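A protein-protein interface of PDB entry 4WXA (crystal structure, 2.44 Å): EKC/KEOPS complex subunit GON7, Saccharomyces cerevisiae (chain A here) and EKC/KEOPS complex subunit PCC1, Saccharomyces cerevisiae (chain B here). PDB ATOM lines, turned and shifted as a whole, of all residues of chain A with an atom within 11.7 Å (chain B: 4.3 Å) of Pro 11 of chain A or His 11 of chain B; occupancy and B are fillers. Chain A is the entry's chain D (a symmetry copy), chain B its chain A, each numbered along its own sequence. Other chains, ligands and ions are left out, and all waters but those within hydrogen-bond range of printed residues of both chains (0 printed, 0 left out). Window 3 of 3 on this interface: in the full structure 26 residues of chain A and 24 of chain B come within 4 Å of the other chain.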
ATOM      1  N   ALA A   6      23.267  12.475 -17.768  1.00  0.00           N
ATOM      2  CA  ALA A   6      23.379  11.565 -16.678  1.00  0.00           C
ATOM      3  C   ALA A   6      24.503  10.573 -16.870  1.00  0.00           C
ATOM      4  O   ALA A   6      24.826  10.213 -17.994  1.00  0.00           O
ATOM      5  CB  ALA A   6      22.089  10.842 -16.530  1.00  0.00           C
ATOM      6  N   GLN A   7      25.106  10.155 -15.759  1.00  0.00           N
ATOM      7  CA  GLN A   7      26.141   9.141 -15.790  1.00  0.00           C
ATOM      8  C   GLN A   7      25.777   8.041 -14.718  1.00  0.00           C
ATOM      9  O   GLN A   7      25.398   8.354 -13.580  1.00  0.00           O
ATOM     10  CB  GLN A   7      27.471   9.822 -15.512  1.00  0.00           C
ATOM     11  CG  GLN A   7      28.698   8.941 -15.349  1.00  0.00           C
ATOM     12  CD  GLN A   7      29.145   8.296 -16.637  1.00  0.00           C
ATOM     13  OE1 GLN A   7      29.107   8.909 -17.722  1.00  0.00           O
ATOM     14  NE2 GLN A   7      29.581   7.060 -16.533  1.00  0.00           N
ATOM     15  N   TYR A   8      25.892   6.785 -15.113  1.00  0.00           N
ATOM     16  CA  TYR A   8      25.578   5.627 -14.250  1.00  0.00           C
ATOM     17  C   TYR A   8      26.794   4.783 -14.058  1.00  0.00           C
ATOM     18  O   TYR A   8      27.579   4.593 -14.956  1.00  0.00           O
ATOM     19  CB  TYR A   8      24.485   4.758 -14.890  1.00  0.00           C
ATOM     20  CG  TYR A   8      24.302   3.353 -14.311  1.00  0.00           C
ATOM     21  CD1 TYR A   8      25.029   2.280 -14.804  1.00  0.00           C
ATOM     22  CD2 TYR A   8      23.401   3.109 -13.294  1.00  0.00           C
ATOM     23  CE1 TYR A   8      24.878   1.004 -14.285  1.00  0.00           C
ATOM     24  CE2 TYR A   8      23.242   1.855 -12.762  1.00  0.00           C
ATOM     25  CZ  TYR A   8      23.981   0.802 -13.277  1.00  0.00           C
ATOM     26  OH  TYR A   8      23.846  -0.439 -12.772  1.00  0.00           O
ATOM     27  N   SER A   9      26.926   4.233 -12.879  1.00  0.00           N
ATOM     28  CA  SER A   9      28.080   3.426 -12.552  1.00  0.00           C
ATOM     29  C   SER A   9      27.646   2.212 -11.686  1.00  0.00           C
ATOM     30  O   SER A   9      26.867   2.370 -10.793  1.00  0.00           O
ATOM     31  CB  SER A   9      28.992   4.354 -11.774  1.00  0.00           C
ATOM     32  OG  SER A   9      30.193   3.736 -11.395  1.00  0.00           O
ATOM     33  N   ALA A  10      28.171   1.034 -11.920  1.00  0.00           N
ATOM     34  CA  ALA A  10      27.802  -0.154 -11.137  1.00  0.00           C
ATOM     35  C   ALA A  10      29.006  -1.029 -10.864  1.00  0.00           C
ATOM     36  O   ALA A  10      29.962  -1.005 -11.615  1.00  0.00           O
ATOM     37  CB  ALA A  10      26.757  -0.952 -11.885  1.00  0.00           C
ATOM     38  N   PRO A  11      28.954  -1.830  -9.803  1.00  0.00           N
ATOM     39  CA  PRO A  11      30.180  -2.483  -9.377  1.00  0.00           C
ATOM     40  C   PRO A  11      30.625  -3.607 -10.278  1.00  0.00           C
ATOM     41  O   PRO A  11      31.671  -4.143 -10.022  1.00  0.00           O
ATOM     42  CB  PRO A  11      29.845  -3.028  -7.967  1.00  0.00           C
ATOM     43  CG  PRO A  11      28.374  -3.029  -7.890  1.00  0.00           C
ATOM     44  CD  PRO A  11      27.844  -2.047  -8.863  1.00  0.00           C
ATOM     45  N   ASP A  12      29.847  -3.997 -11.283  1.00  0.00           N
ATOM     46  CA  ASP A  12      30.334  -4.980 -12.259  1.00  0.00           C
ATOM     47  C   ASP A  12      31.217  -4.313 -13.335  1.00  0.00           C
ATOM     48  O   ASP A  12      31.525  -4.916 -14.315  1.00  0.00           O
ATOM     49  CB  ASP A  12      29.179  -5.777 -12.934  1.00  0.00           C
ATOM     50  CG  ASP A  12      28.181  -4.880 -13.702  1.00  0.00           C
ATOM     51  OD1 ASP A  12      28.062  -3.682 -13.351  1.00  0.00           O
ATOM     52  OD2 ASP A  12      27.491  -5.361 -14.639  1.00  0.00           O
ATOM     53  N   GLY A  13      31.589  -3.057 -13.168  1.00  0.00           N
ATOM     54  CA  GLY A  13      32.544  -2.445 -14.052  1.00  0.00           C
ATOM     55  C   GLY A  13      31.904  -1.692 -15.178  1.00  0.00           C
ATOM     56  O   GLY A  13      32.571  -1.320 -16.100  1.00  0.00           O
ATOM     57  N   VAL A  14      30.608  -1.473 -15.104  1.00  0.00           N
ATOM     58  CA  VAL A  14      29.846  -0.863 -16.176  1.00  0.00           C
ATOM     59  C   VAL A  14      29.673   0.636 -15.949  1.00  0.00           C
ATOM     60  O   VAL A  14      29.339   1.054 -14.861  1.00  0.00           O
ATOM     61  CB  VAL A  14      28.479  -1.554 -16.291  1.00  0.00           C
ATOM     62  CG1 VAL A  14      27.507  -0.791 -17.169  1.00  0.00           C
ATOM     63  CG2 VAL A  14      28.697  -2.956 -16.825  1.00  0.00           C
ATOM     64  N   GLU A  15      29.905   1.445 -16.985  1.00  0.00           N
ATOM     65  CA  GLU A  15      29.736   2.917 -16.841  1.00  0.00           C
ATOM     66  C   GLU A  15      28.906   3.323 -17.998  1.00  0.00           C
ATOM     67  O   GLU A  15      29.169   2.916 -19.089  1.00  0.00           O
ATOM     68  CB  GLU A  15      31.060   3.640 -16.932  1.00  0.00           C
ATOM     69  CG  GLU A  15      32.074   3.359 -15.834  1.00  0.00           C
ATOM     70  CD  GLU A  15      31.822   4.189 -14.617  1.00  0.00           C
ATOM     71  N   LYS A  16      27.892   4.119 -17.787  1.00  0.00           N
ATOM     72  CA  LYS A  16      26.970   4.375 -18.865  1.00  0.00           C
ATOM     73  C   LYS A  16      26.632   5.846 -18.870  1.00  0.00           C
ATOM     74  O   LYS A  16      26.160   6.368 -17.861  1.00  0.00           O
ATOM     75  CB  LYS A  16      25.734   3.553 -18.642  1.00  0.00           C
ATOM     76  CG  LYS A  16      24.526   3.970 -19.433  1.00  0.00           C
ATOM     77  CD  LYS A  16      24.727   3.801 -20.922  1.00  0.00           C
ATOM     78  CE  LYS A  16      23.403   3.872 -21.630  1.00  0.00           C
ATOM     79  NZ  LYS A  16      23.601   4.223 -23.041  1.00  0.00           N
ATOM     80  N   PHE A  18      24.347   8.992 -20.486  1.00  0.00           N
ATOM     81  CA  PHE A  18      23.124   9.383 -21.150  1.00  0.00           C
ATOM     82  C   PHE A  18      23.158  10.830 -21.631  1.00  0.00           C
ATOM     83  O   PHE A  18      23.582  11.746 -20.919  1.00  0.00           O
ATOM     84  CB  PHE A  18      21.988   9.287 -20.173  1.00  0.00           C
ATOM     85  CG  PHE A  18      21.787   7.927 -19.577  1.00  0.00           C
ATOM     86  CD1 PHE A  18      22.414   7.572 -18.417  1.00  0.00           C
ATOM     87  CD2 PHE A  18      20.915   7.032 -20.148  1.00  0.00           C
ATOM     88  CE1 PHE A  18      22.217   6.318 -17.850  1.00  0.00           C
ATOM     89  CE2 PHE A  18      20.690   5.804 -19.579  1.00  0.00           C
ATOM     90  CZ  PHE A  18      21.342   5.434 -18.425  1.00  0.00           C
ATOM     91  N   ILE A  81      16.946   6.151 -19.068  1.00  0.00           N
ATOM     92  CA  ILE A  81      17.376   5.575 -17.802  1.00  0.00           C
ATOM     93  C   ILE A  81      16.505   4.360 -17.493  1.00  0.00           C
ATOM     94  O   ILE A  81      17.009   3.313 -17.126  1.00  0.00           O
ATOM     95  CB  ILE A  81      17.298   6.619 -16.689  1.00  0.00           C
ATOM     96  CG1 ILE A  81      18.419   7.644 -16.863  1.00  0.00           C
ATOM     97  CG2 ILE A  81      17.520   6.062 -15.294  1.00  0.00           C
ATOM     98  CD1 ILE A  81      18.140   8.999 -16.232  1.00  0.00           C
ATOM     99  N   PHE A  84      17.298   1.548 -19.798  1.00  0.00           N
ATOM    100  CA  PHE A  84      18.597   0.952 -19.511  1.00  0.00           C
ATOM    101  C   PHE A  84      18.554   0.053 -18.270  1.00  0.00           C
ATOM    102  O   PHE A  84      19.194  -0.997 -18.227  1.00  0.00           O
ATOM    103  CB  PHE A  84      19.663   2.064 -19.340  1.00  0.00           C
ATOM    104  CG  PHE A  84      20.992   1.556 -18.878  1.00  0.00           C
ATOM    105  CD1 PHE A  84      21.867   0.986 -19.757  1.00  0.00           C
ATOM    106  CD2 PHE A  84      21.332   1.626 -17.533  1.00  0.00           C
ATOM    107  CE1 PHE A  84      23.071   0.496 -19.310  1.00  0.00           C
ATOM    108  CE2 PHE A  84      22.531   1.121 -17.080  1.00  0.00           C
ATOM    109  CZ  PHE A  84      23.398   0.536 -17.964  1.00  0.00           C
ATOM    110  N   LEU A  85      17.833   0.495 -17.242  1.00  0.00           N
ATOM    111  CA  LEU A  85      17.857  -0.202 -15.971  1.00  0.00           C
ATOM    112  C   LEU A  85      17.004  -1.451 -16.094  1.00  0.00           C
ATOM    113  O   LEU A  85      17.355  -2.517 -15.572  1.00  0.00           O
ATOM    114  CB  LEU A  85      17.377   0.698 -14.837  1.00  0.00           C
ATOM    115  CG  LEU A  85      18.333   1.841 -14.442  1.00  0.00           C
ATOM    116  CD1 LEU A  85      17.688   2.822 -13.466  1.00  0.00           C
ATOM    117  CD2 LEU A  85      19.592   1.268 -13.818  1.00  0.00           C
ATOM    118  N   THR A  86      15.893  -1.323 -16.805  1.00  0.00           N
ATOM    119  CA  THR A  86      15.017  -2.452 -17.011  1.00  0.00           C
ATOM    120  C   THR A  86      15.789  -3.575 -17.719  1.00  0.00           C
ATOM    121  O   THR A  86      15.797  -4.713 -17.253  1.00  0.00           O
ATOM    122  CB  THR A  86      13.754  -2.024 -17.771  1.00  0.00           C
ATOM    123  OG1 THR A  86      13.072  -1.061 -16.971  1.00  0.00           O
ATOM    124  CG2 THR A  86      12.818  -3.223 -18.012  1.00  0.00           C
ATOM    125  N   GLY A  87      16.479  -3.221 -18.800  1.00  0.00           N
ATOM    126  CA  GLY A  87      17.391  -4.135 -19.476  1.00  0.00           C
ATOM    127  C   GLY A  87      18.415  -4.782 -18.558  1.00  0.00           C
ATOM    128  O   GLY A  87      18.761  -5.928 -18.731  1.00  0.00           O
ATOM    129  N   ARG A  88      18.928  -4.043 -17.591  1.00  0.00           N
ATOM    130  CA  ARG A  88      19.905  -4.610 -16.694  1.00  0.00           C
ATOM    131  C   ARG A  88      19.232  -5.636 -15.836  1.00  0.00           C
ATOM    132  O   ARG A  88      19.844  -6.635 -15.513  1.00  0.00           O
ATOM    133  CB  ARG A  88      20.537  -3.565 -15.788  1.00  0.00           C
ATOM    134  CG  ARG A  88      21.352  -2.468 -16.509  1.00  0.00           C
ATOM    135  CD  ARG A  88      22.828  -2.772 -16.509  1.00  0.00           C
ATOM    136  NE  ARG A  88      23.372  -2.781 -15.166  1.00  0.00           N
ATOM    137  CZ  ARG A  88      24.563  -3.279 -14.845  1.00  0.00           C
ATOM    138  NH1 ARG A  88      25.355  -3.843 -15.752  1.00  0.00           N
ATOM    139  NH2 ARG A  88      24.971  -3.227 -13.594  1.00  0.00           N
ATOM    140  N   MET A  89      17.989  -5.382 -15.433  1.00  0.00           N
ATOM    141  CA  MET A  89      17.249  -6.351 -14.614  1.00  0.00           C
ATOM    142  C   MET A  89      16.887  -7.602 -15.458  1.00  0.00           C
ATOM    143  O   MET A  89      17.106  -8.717 -15.032  1.00  0.00           O
ATOM    144  CB  MET A  89      15.992  -5.736 -14.030  1.00  0.00           C
ATOM    145  CG  MET A  89      16.205  -4.922 -12.763  1.00  0.00           C
ATOM    146  SD  MET A  89      14.726  -3.928 -12.435  1.00  0.00           S
ATOM    147  CE  MET A  89      14.966  -2.589 -13.582  1.00  0.00           C
ATOM    148  N   GLU A  90      16.365  -7.399 -16.667  1.00  0.00           N
ATOM    149  CA  GLU A  90      16.038  -8.497 -17.544  1.00  0.00           C
ATOM    150  C   GLU A  90      17.241  -9.431 -17.766  1.00  0.00           C
ATOM    151  O   GLU A  90      17.075 -10.628 -17.747  1.00  0.00           O
ATOM    152  CB  GLU A  90      15.386  -8.004 -18.867  1.00  0.00           C
ATOM    153  CG  GLU A  90      13.912  -7.547 -18.687  1.00  0.00           C
ATOM    154  CD  GLU A  90      13.314  -6.728 -19.842  1.00  0.00           C
ATOM    155  N   LEU A  91      18.452  -8.925 -17.927  1.00  0.00           N
ATOM    156  CA  LEU A  91      19.617  -9.825 -18.051  1.00  0.00           C
ATOM    157  C   LEU A  91      20.024 -10.507 -16.746  1.00  0.00           C
ATOM    158  O   LEU A  91      20.552 -11.610 -16.791  1.00  0.00           O
ATOM    159  CB  LEU A  91      20.856  -9.098 -18.590  1.00  0.00           C
ATOM    160  CG  LEU A  91      20.858  -8.679 -20.055  1.00  0.00           C
ATOM    161  CD1 LEU A  91      22.113  -7.869 -20.376  1.00  0.00           C
ATOM    162  CD2 LEU A  91      20.699  -9.885 -20.982  1.00  0.00           C
ATOM    163  N   ALA A  92      19.834  -9.844 -15.607  1.00  0.00           N
ATOM    164  CA  ALA A  92      20.177 -10.449 -14.319  1.00  0.00           C
ATOM    165  C   ALA A  92      19.240 -11.631 -14.009  1.00  0.00           C
ATOM    166  O   ALA A  92      19.676 -12.630 -13.438  1.00  0.00           O
ATOM    167  CB  ALA A  92      20.134  -9.421 -13.209  1.00  0.00           C
ATOM    168  N   LEU B   9      26.006   0.705  -1.230  1.00  0.00           N
ATOM    169  CA  LEU B   9      25.237   1.627  -2.056  1.00  0.00           C
ATOM    170  C   LEU B   9      26.107   1.970  -3.238  1.00  0.00           C
ATOM    171  O   LEU B   9      26.634   3.034  -3.328  1.00  0.00           O
ATOM    172  CB  LEU B   9      24.766   2.870  -1.278  1.00  0.00           C
ATOM    173  CG  LEU B   9      23.641   2.646  -0.223  1.00  0.00           C
ATOM    174  CD1 LEU B   9      23.405   3.893   0.592  1.00  0.00           C
ATOM    175  CD2 LEU B   9      22.307   2.291  -0.838  1.00  0.00           C
ATOM    176  N   ASP B  10      26.261   1.030  -4.141  1.00  0.00           N
ATOM    177  CA  ASP B  10      27.307   1.132  -5.121  1.00  0.00           C
ATOM    178  C   ASP B  10      26.817   1.107  -6.575  1.00  0.00           C
ATOM    179  O   ASP B  10      27.620   1.054  -7.459  1.00  0.00           O
ATOM    180  CB  ASP B  10      28.340   0.041  -4.864  1.00  0.00           C
ATOM    181  CG  ASP B  10      27.746  -1.377  -4.839  1.00  0.00           C
ATOM    182  OD1 ASP B  10      26.516  -1.592  -5.133  1.00  0.00           O
ATOM    183  OD2 ASP B  10      28.568  -2.289  -4.547  1.00  0.00           O
ATOM    184  N   HIS B  11      25.502   1.089  -6.795  1.00  0.00           N
ATOM    185  CA  HIS B  11      24.911   1.434  -8.066  1.00  0.00           C
ATOM    186  C   HIS B  11      24.545   2.931  -8.062  1.00  0.00           C
ATOM    187  O   HIS B  11      23.690   3.363  -7.329  1.00  0.00           O
ATOM    188  CB  HIS B  11      23.665   0.645  -8.246  1.00  0.00           C
ATOM    189  CG  HIS B  11      23.895  -0.821  -8.464  1.00  0.00           C
ATOM    190  ND1 HIS B  11      24.337  -1.673  -7.465  1.00  0.00           N
ATOM    191  CD2 HIS B  11      23.683  -1.594  -9.556  1.00  0.00           C
ATOM    192  CE1 HIS B  11      24.415  -2.905  -7.952  1.00  0.00           C
ATOM    193  NE2 HIS B  11      24.010  -2.884  -9.212  1.00  0.00           N
ATOM    194  N   THR B  12      25.217   3.735  -8.855  1.00  0.00           N
ATOM    195  CA  THR B  12      25.095   5.196  -8.734  1.00  0.00           C
ATOM    196  C   THR B  12      24.717   5.797 -10.025  1.00  0.00           C
ATOM    197  O   THR B  12      25.058   5.290 -11.086  1.00  0.00           O
ATOM    198  CB  THR B  12      26.382   5.883  -8.243  1.00  0.00           C
ATOM    199  OG1 THR B  12      27.417   5.727  -9.179  1.00  0.00           O
ATOM    200  CG2 THR B  12      26.895   5.218  -6.965  1.00  0.00           C
ATOM    201  N   PHE B  58      22.267  10.008  -7.031  1.00  0.00           N
ATOM    202  CA  PHE B  58      21.648   8.802  -6.435  1.00  0.00           C
ATOM    203  C   PHE B  58      22.679   7.712  -6.150  1.00  0.00           C
ATOM    204  O   PHE B  58      23.653   7.563  -6.887  1.00  0.00           O
ATOM    205  CB  PHE B  58      20.634   8.232  -7.408  1.00  0.00           C
ATOM    206  CG  PHE B  58      19.673   9.239  -7.943  1.00  0.00           C
ATOM    207  CD1 PHE B  58      20.010  10.025  -9.015  1.00  0.00           C
ATOM    208  CD2 PHE B  58      18.420   9.399  -7.378  1.00  0.00           C
ATOM    209  CE1 PHE B  58      19.114  10.978  -9.534  1.00  0.00           C
ATOM    210  CE2 PHE B  58      17.528  10.331  -7.874  1.00  0.00           C
ATOM    211  CZ  PHE B  58      17.887  11.135  -8.966  1.00  0.00           C
ATOM    212  N   ARG B  59      22.447   6.951  -5.105  1.00  0.00           N
ATOM    213  CA  ARG B  59      23.241   5.791  -4.712  1.00  0.00           C
ATOM    214  C   ARG B  59      22.224   4.754  -4.279  1.00  0.00           C
ATOM    215  O   ARG B  59      21.253   5.080  -3.567  1.00  0.00           O
ATOM    216  CB  ARG B  59      24.176   6.091  -3.549  1.00  0.00           C
ATOM    217  CG  ARG B  59      25.089   7.276  -3.804  1.00  0.00           C
ATOM    218  CD  ARG B  59      26.164   7.491  -2.738  1.00  0.00           C
ATOM    219  NE  ARG B  59      25.636   8.206  -1.576  1.00  0.00           N
ATOM    220  CZ  ARG B  59      25.246   9.485  -1.602  1.00  0.00           C
ATOM    221  N   SER B  60      22.406   3.505  -4.698  1.00  0.00           N
ATOM    222  CA  SER B  60      21.416   2.459  -4.374  1.00  0.00           C
ATOM    223  C   SER B  60      22.047   1.103  -4.321  1.00  0.00           C
ATOM    224  O   SER B  60      23.120   0.887  -4.869  1.00  0.00           O
ATOM    225  CB  SER B  60      20.360   2.468  -5.448  1.00  0.00           C
ATOM    226  OG  SER B  60      19.356   1.531  -5.195  1.00  0.00           O
ATOM    227  N   ILE B  61      21.385   0.177  -3.664  1.00  0.00           N
ATOM    228  CA  ILE B  61      21.935  -1.175  -3.551  1.00  0.00           C
ATOM    229  C   ILE B  61      21.766  -2.002  -4.807  1.00  0.00           C
ATOM    230  O   ILE B  61      22.492  -2.988  -4.973  1.00  0.00           O
ATOM    231  CB  ILE B  61      21.331  -1.997  -2.406  1.00  0.00           C
ATOM    232  CG1 ILE B  61      19.817  -2.093  -2.549  1.00  0.00           C
ATOM    233  CG2 ILE B  61      21.789  -1.406  -1.083  1.00  0.00           C
ATOM    234  CD1 ILE B  61      19.193  -3.158  -1.648  1.00  0.00           C
ATOM    235  N   ASP B  62      20.816  -1.625  -5.669  1.00  0.00           N
ATOM    236  CA  ASP B  62      20.631  -2.372  -6.903  1.00  0.00           C
ATOM    237  C   ASP B  62      19.811  -1.616  -7.879  1.00  0.00           C
ATOM    238  O   ASP B  62      19.311  -0.545  -7.568  1.00  0.00           O
ATOM    239  CB  ASP B  62      20.030  -3.769  -6.639  1.00  0.00           C
ATOM    240  CG  ASP B  62      18.572  -3.718  -6.212  1.00  0.00           C
ATOM    241  OD1 ASP B  62      17.819  -2.828  -6.687  1.00  0.00           O
ATOM    242  OD2 ASP B  62      18.167  -4.608  -5.421  1.00  0.00           O
ATOM    243  N   ASP B  63      19.680  -2.188  -9.064  1.00  0.00           N
ATOM    244  CA  ASP B  63      19.077  -1.490 -10.180  1.00  0.00           C
ATOM    245  C   ASP B  63      17.583  -1.326 -10.017  1.00  0.00           C
ATOM    246  O   ASP B  63      16.992  -0.384 -10.559  1.00  0.00           O
ATOM    247  CB  ASP B  63      19.406  -2.211 -11.508  1.00  0.00           C
ATOM    248  CG  ASP B  63      20.833  -1.950 -11.988  1.00  0.00           C
ATOM    249  OD1 ASP B  63      21.380  -0.905 -11.677  1.00  0.00           O
ATOM    250  OD2 ASP B  63      21.435  -2.764 -12.686  1.00  0.00           O
ATOM    251  N   LEU B  66      17.049   1.620  -7.630  1.00  0.00           N
ATOM    252  CA  LEU B  66      17.420   2.815  -8.394  1.00  0.00           C
ATOM    253  C   LEU B  66      16.311   3.215  -9.360  1.00  0.00           C
ATOM    254  O   LEU B  66      15.904   4.380  -9.366  1.00  0.00           O
ATOM    255  CB  LEU B  66      18.750   2.599  -9.104  1.00  0.00           C
ATOM    256  CG  LEU B  66      19.459   3.813  -9.657  1.00  0.00           C
ATOM    257  CD1 LEU B  66      19.956   4.718  -8.527  1.00  0.00           C
ATOM    258  CD2 LEU B  66      20.627   3.380 -10.496  1.00  0.00           C
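OD2 of Asp 63 of chain B is in salt-bridge range of NE of Arg 88 of chain A (3.1 Å). O of Thr 12 of chain B sits at hydrogen-bond distance from N of Ser 9 of chain A (2.8 Å). OH of Tyr 8 of chain A is in hydrogen-bond range of OD1 of Asp 63 of chain B (2.7 Å).
N of Ser 60 of chain B is in hydrogen-bond range of O of His 11 of chain B (2.9 Å). The guanidinium group (NH1) of Arg 88 of chain A lies within salt-bridge range of the side-chain carboxylate (OD2) of Asp 12 of chain A (2.8 Å). The side-chain carboxylate (OD1) of Asp 10 of chain B sits at hydrogen-bond distance from a ring nitrogen (ND1) of His 11 of chain B (3.2 Å). The side-chain hydroxyl (OG) of Ser 60 of chain B lies within hydrogen-bond range of the backbone NH (N) of Leu 66 of chain B, 3.4 Å away. The side-chain hydroxyl (OH) of Tyr 8 of chain A sits at hydrogen-bond distance from the guanidinium group (NH2) of Arg 88 of chain A (3.1 Å). O of Ile 61 of chain B is in hydrogen-bond range of ND1 of His 11 of chain B, 3.4 Å away.
Among the printed residues, merely in contact across the chains: Tyr 8 of chain A with Thr 12 of chain B, Pro 11 of chain A with Asp 10 of chain B, Tyr 8 of chain A with His 11 of chain B, Ser 9 of chain A with His 11 of chain B, Leu 85 of chain A with Asp 63 of chain B, Pro 11 of chain A with His 11 of chain B, Ser 9 of chain A with Asp 10 of chain B, Tyr 8 of chain A with Leu 66 of chain B, Ala 10 of chain A with Asp 10 of chain B, Ala 10 of chain A with His 11 of chain B and Gln 7 of chain A with Thr 12 of chain B.
Printed residues of chain B within 4 Å of Gln 7 of chain A: Thr 12. Printed residues of chain B within 4 Å of Tyr 8 of chain A: His 11 (3.4 Å), Thr 12 (3.2 Å), Asp 63 (2.7 Å) and Leu 66 (3.8 Å). Printed residues of chain B within 4 Å of Ser 9 of chain A: Asp 10 (3.7 Å), His 11 (3.5 Å) and Thr 12 (2.8 Å). Pro 11 of chain A touches just these residues of chain B: Asp 10 and His 11. Asp 10 of chain B touches just these residues of chain A: Ser 9 (3.7 Å), Ala 10 (3.9 Å) and Pro 11 (3.4 Å). Of chain A, only Gln 7, Tyr 8 and Ser 9 come within 4 Å of Thr 12 of chain B. No residue of chain A comes within 4 Å of Ser 60 of chain B. Of chain A, only Tyr 8, Leu 85 and Arg 88 come within 4 Å of Asp 63 of chain B. Of the printed residues of chain A, Leu 66 of chain B touches Tyr 8 (3.8 Å).
Hydrophobic or aromatic side chains of chain A within 4 Å of the printed part of chain B: Tyr 8, Ala 10, Pro 11 and Leu 85. Along chain A the printed residues that touch a printed residue of chain B span positions 7 to 88. Of the 11 printed residues of chain B, 5 touch a printed residue of chain A. Printed residues of chain B that touch a printed residue of chain A: Asp 10, His 11, Thr 12, Asp 63 and Leu 66. Hydrophobic or aromatic side chains of chain B within 4 Å of the printed part of chain A: His 11 and Leu 66.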
